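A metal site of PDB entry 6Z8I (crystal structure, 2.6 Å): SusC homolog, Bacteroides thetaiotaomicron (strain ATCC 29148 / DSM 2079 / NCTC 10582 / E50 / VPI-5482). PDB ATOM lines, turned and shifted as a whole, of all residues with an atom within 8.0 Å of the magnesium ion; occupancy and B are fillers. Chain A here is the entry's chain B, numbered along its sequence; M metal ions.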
ATOM      1  N   ALA A 848       7.046  13.707  27.040  1.00  0.00           N
ATOM      2  CA  ALA A 848       7.655  12.392  27.116  1.00  0.00           C
ATOM      3  C   ALA A 848       7.038  11.595  28.260  1.00  0.00           C
ATOM      4  O   ALA A 848       6.719  12.141  29.320  1.00  0.00           O
ATOM      5  CB  ALA A 848       9.172  12.500  27.319  1.00  0.00           C
ATOM      6  N   THR A 849       6.821  10.305  28.013  1.00  0.00           N
ATOM      7  CA  THR A 849       6.125   9.474  28.980  1.00  0.00           C
ATOM      8  C   THR A 849       7.004   9.284  30.211  1.00  0.00           C
ATOM      9  O   THR A 849       8.149   8.828  30.104  1.00  0.00           O
ATOM     10  CB  THR A 849       5.739   8.127  28.347  1.00  0.00           C
ATOM     11  OG1 THR A 849       6.812   7.640  27.536  1.00  0.00           O
ATOM     12  CG2 THR A 849       4.490   8.298  27.456  1.00  0.00           C
ATOM     13  N   ARG A 861      12.572  17.108  32.279  1.00  0.00           N
ATOM     14  CA  ARG A 861      12.867  17.336  30.874  1.00  0.00           C
ATOM     15  C   ARG A 861      13.443  16.103  30.210  1.00  0.00           C
ATOM     16  O   ARG A 861      14.132  15.276  30.830  1.00  0.00           O
ATOM     17  CB  ARG A 861      13.839  18.511  30.702  1.00  0.00           C
ATOM     18  CG  ARG A 861      13.902  19.033  29.280  1.00  0.00           C
ATOM     19  CD  ARG A 861      15.026  20.038  29.098  1.00  0.00           C
ATOM     20  NE  ARG A 861      14.801  21.270  29.836  1.00  0.00           N
ATOM     21  CZ  ARG A 861      15.696  22.251  29.898  1.00  0.00           C
ATOM     22  NH1 ARG A 861      16.863  22.110  29.269  1.00  0.00           N
ATOM     23  NH2 ARG A 861      15.434  23.354  30.591  1.00  0.00           N
ATOM     24  N   ASP A 862      13.150  15.976  28.909  1.00  0.00           N
ATOM     25  CA  ASP A 862      13.592  14.885  28.056  1.00  0.00           C
ATOM     26  C   ASP A 862      14.886  15.304  27.358  1.00  0.00           C
ATOM     27  O   ASP A 862      14.906  15.703  26.205  1.00  0.00           O
ATOM     28  CB  ASP A 862      12.485  14.544  27.068  1.00  0.00           C
ATOM     29  CG  ASP A 862      12.794  13.312  26.224  1.00  0.00           C
ATOM     30  OD1 ASP A 862      13.548  12.417  26.704  1.00  0.00           O
ATOM     31  OD2 ASP A 862      12.253  13.249  25.079  1.00  0.00           O
ATOM     32  N   ILE A 863      15.995  15.175  28.101  1.00  0.00           N
ATOM     33  CA  ILE A 863      17.269  15.798  27.700  1.00  0.00           C
ATOM     34  C   ILE A 863      17.715  15.307  26.337  1.00  0.00           C
ATOM     35  O   ILE A 863      18.267  16.074  25.538  1.00  0.00           O
ATOM     36  CB  ILE A 863      18.363  15.533  28.769  1.00  0.00           C
ATOM     37  CG1 ILE A 863      18.389  16.605  29.871  1.00  0.00           C
ATOM     38  CG2 ILE A 863      19.736  15.479  28.135  1.00  0.00           C
ATOM     39  CD1 ILE A 863      17.076  17.022  30.426  1.00  0.00           C
ATOM     40  N   ASP A 864      17.471  14.031  26.024  1.00  0.00           N
ATOM     41  CA  ASP A 864      17.957  13.395  24.803  1.00  0.00           C
ATOM     42  C   ASP A 864      16.874  13.219  23.735  1.00  0.00           C
ATOM     43  O   ASP A 864      17.175  12.726  22.651  1.00  0.00           O
ATOM     44  CB  ASP A 864      18.568  12.027  25.115  1.00  0.00           C
ATOM     45  CG  ASP A 864      17.569  11.033  25.725  1.00  0.00           C
ATOM     46  OD1 ASP A 864      16.369  11.362  25.887  1.00  0.00           O
ATOM     47  OD2 ASP A 864      17.988   9.901  26.048  1.00  0.00           O
ATOM     48  N   HIS A 865      15.627  13.604  24.029  1.00  0.00           N
ATOM     49  CA  HIS A 865      14.562  13.641  23.042  1.00  0.00           C
ATOM     50  C   HIS A 865      14.185  12.250  22.513  1.00  0.00           C
ATOM     51  O   HIS A 865      13.835  12.114  21.344  1.00  0.00           O
ATOM     52  CB  HIS A 865      14.927  14.549  21.860  1.00  0.00           C
ATOM     53  CG  HIS A 865      15.164  15.970  22.251  1.00  0.00           C
ATOM     54  ND1 HIS A 865      16.435  16.497  22.401  1.00  0.00           N
ATOM     55  CD2 HIS A 865      14.302  16.985  22.511  1.00  0.00           C
ATOM     56  CE1 HIS A 865      16.338  17.766  22.754  1.00  0.00           C
ATOM     57  NE2 HIS A 865      15.062  18.086  22.820  1.00  0.00           N
ATOM     58  N   ASN A 866      14.234  11.217  23.356  1.00  0.00           N
ATOM     59  CA  ASN A 866      13.801   9.879  22.938  1.00  0.00           C
ATOM     60  C   ASN A 866      12.318   9.653  23.140  1.00  0.00           C
ATOM     61  O   ASN A 866      11.812   8.618  22.692  1.00  0.00           O
ATOM     62  CB  ASN A 866      14.576   8.778  23.680  1.00  0.00           C
ATOM     63  CG  ASN A 866      14.592   8.958  25.184  1.00  0.00           C
ATOM     64  OD1 ASN A 866      13.917   9.843  25.735  1.00  0.00           O
ATOM     65  ND2 ASN A 866      15.370   8.134  25.871  1.00  0.00           N
ATOM     66  N   GLY A 867      11.616  10.567  23.817  1.00  0.00           N
ATOM     67  CA  GLY A 867      10.202  10.405  24.102  1.00  0.00           C
ATOM     68  C   GLY A 867       9.870   9.708  25.398  1.00  0.00           C
ATOM     69  O   GLY A 867       8.688   9.465  25.675  1.00  0.00           O
ATOM     70  N   VAL A 868      10.873   9.352  26.197  1.00  0.00           N
ATOM     71  CA  VAL A 868      10.642   8.873  27.547  1.00  0.00           C
ATOM     72  C   VAL A 868      11.586   9.596  28.498  1.00  0.00           C
ATOM     73  O   VAL A 868      12.695  10.001  28.122  1.00  0.00           O
ATOM     74  CB  VAL A 868      10.828   7.347  27.693  1.00  0.00           C
ATOM     75  CG1 VAL A 868       9.591   6.605  27.259  1.00  0.00           C
ATOM     76  CG2 VAL A 868      12.034   6.897  26.915  1.00  0.00           C
ATOM     77  N   ILE A 869      11.133   9.723  29.744  1.00  0.00           N
ATOM     78  CA  ILE A 869      11.950  10.211  30.839  1.00  0.00           C
ATOM     79  C   ILE A 869      12.458   8.992  31.596  1.00  0.00           C
ATOM     80  O   ILE A 869      11.679   8.260  32.211  1.00  0.00           O
ATOM     81  CB  ILE A 869      11.158  11.152  31.754  1.00  0.00           C
ATOM     82  CG1 ILE A 869      10.389  12.172  30.923  1.00  0.00           C
ATOM     83  CG2 ILE A 869      12.076  11.838  32.761  1.00  0.00           C
ATOM     84  CD1 ILE A 869      11.268  13.255  30.298  1.00  0.00           C
ATOM     85  N   ASP A 870      13.768   8.734  31.535  1.00  0.00           N
ATOM     86  CA  ASP A 870      14.383   7.682  32.318  1.00  0.00           C
ATOM     87  C   ASP A 870      15.748   8.180  32.781  1.00  0.00           C
ATOM     88  O   ASP A 870      16.024   9.395  32.766  1.00  0.00           O
ATOM     89  CB  ASP A 870      14.435   6.343  31.541  1.00  0.00           C
ATOM     90  CG  ASP A 870      15.259   6.435  30.266  1.00  0.00           C
ATOM     91  OD1 ASP A 870      15.304   5.419  29.532  1.00  0.00           O
ATOM     92  OD2 ASP A 870      15.843   7.496  29.965  1.00  0.00           O
ATOM     93  N   GLU A 871      16.626   7.251  33.203  1.00  0.00           N
ATOM     94  CA  GLU A 871      17.836   7.609  33.924  1.00  0.00           C
ATOM     95  C   GLU A 871      18.854   8.380  33.078  1.00  0.00           C
ATOM     96  O   GLU A 871      19.779   8.988  33.630  1.00  0.00           O
ATOM     97  CB  GLU A 871      18.514   6.349  34.500  1.00  0.00           C
ATOM     98  CG  GLU A 871      17.711   5.598  35.548  1.00  0.00           C
ATOM     99  CD  GLU A 871      16.767   4.590  34.929  1.00  0.00           C
ATOM    100  OE1 GLU A 871      16.790   4.428  33.686  1.00  0.00           O
ATOM    101  OE2 GLU A 871      15.989   3.966  35.684  1.00  0.00           O
ATOM    102  N   ARG A 872      18.710   8.360  31.750  1.00  0.00           N
ATOM    103  CA  ARG A 872      19.616   9.136  30.914  1.00  0.00           C
ATOM    104  C   ARG A 872      19.222  10.606  30.843  1.00  0.00           C
ATOM    105  O   ARG A 872      20.060  11.438  30.501  1.00  0.00           O
ATOM    106  CB  ARG A 872      19.673   8.534  29.503  1.00  0.00           C
ATOM    107  CG  ARG A 872      20.201   7.102  29.485  1.00  0.00           C
ATOM    108  CD  ARG A 872      19.820   6.319  28.201  1.00  0.00           C
ATOM    109  NE  ARG A 872      18.370   6.200  28.001  1.00  0.00           N
ATOM    110  CZ  ARG A 872      17.822   5.624  26.937  1.00  0.00           C
ATOM    111  NH1 ARG A 872      18.579   5.098  25.977  1.00  0.00           N
ATOM    112  NH2 ARG A 872      16.495   5.556  26.818  1.00  0.00           N
ATOM    113  N   ASP A 873      17.974  10.950  31.178  1.00  0.00           N
ATOM    114  CA  ASP A 873      17.513  12.336  31.067  1.00  0.00           C
ATOM    115  C   ASP A 873      18.059  13.188  32.217  1.00  0.00           C
ATOM    116  O   ASP A 873      17.329  13.857  32.945  1.00  0.00           O
ATOM    117  CB  ASP A 873      15.989  12.391  31.002  1.00  0.00           C
ATOM    118  CG  ASP A 873      15.446  11.749  29.727  1.00  0.00           C
ATOM    119  OD1 ASP A 873      14.749  10.718  29.824  1.00  0.00           O
ATOM    120  OD2 ASP A 873      15.726  12.253  28.609  1.00  0.00           O
ATOM    121  N   GLN A 874      19.382  13.162  32.326  1.00  0.00           N
ATOM    122  CA  GLN A 874      20.138  13.916  33.323  1.00  0.00           C
ATOM    123  C   GLN A 874      21.315  14.649  32.679  1.00  0.00           C
ATOM    124  O   GLN A 874      21.844  14.221  31.645  1.00  0.00           O
ATOM    125  CB  GLN A 874      20.662  12.994  34.423  1.00  0.00           C
ATOM    126  CG  GLN A 874      19.588  12.499  35.376  1.00  0.00           C
ATOM    127  CD  GLN A 874      20.165  11.546  36.405  1.00  0.00           C
ATOM    128  OE1 GLN A 874      20.659  11.977  37.452  1.00  0.00           O
ATOM    129  NE2 GLN A 874      20.155  10.249  36.103  1.00  0.00           N
HETATM  130 MG    MG M   1      15.188  10.357  27.440  1.00  0.00          MG
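The side-chain carboxylate of Asp 873 sits close to the backbone NH of Ile 863 (3.0 Å).
The side-chain amide oxygen (OD1) of Asn 866 sits close to the backbone carbonyl oxygen (O) of Val 868, 2.7 Å away.
ND2 of Asn 866 sits close to NH2 of Arg 872, at 3.0 Å.
The side-chain carboxylate (OD2) of Asp 862 lies within hydrogen-bond range of the backbone NH (N) of Gly 867, at 3.0 Å.
The backbone NH (N) of Asp 870 lies close to the side-chain carboxylate (OD1) of Asp 873 (2.8 Å).
The side-chain carboxylate (OD1) of Asp 870 is in salt-bridge range of the guanidinium group (NH2) of Arg 872, at 3.0 Å.
N of Asn 866 lies within hydrogen-bond range of OD2 of Asp 862 (3.3 Å).
Residues that only touch the magnesium ion: Asp 870 (3.9 Å).
Of the 16 residues printed, 6 come within 4 Å of the magnesium ion.
The magnesium ion is bound by the side-chain amide oxygen (OD1) of Asn 866 (2.2 Å), the side-chain carboxylate (OD1) of Asp 864 (2.2 Å), the side-chain carboxylate (OD2) of Asp 873 (2.3 Å) and the side-chain carboxylate (OD1) of Asp 873 (2.5 Å).
The magnesium ion has four donor atoms within binding distance.
Slightly farther from the magnesium ion lies O of Val 868 (2.6 Å).
Slightly farther from the magnesium ion lies the side-chain amide nitrogen (ND2) of Asn 866 (2.7 Å).
Slightly farther from the magnesium ion lies the side-chain carboxylate (OD1) of Asp 862 (2.7 Å).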
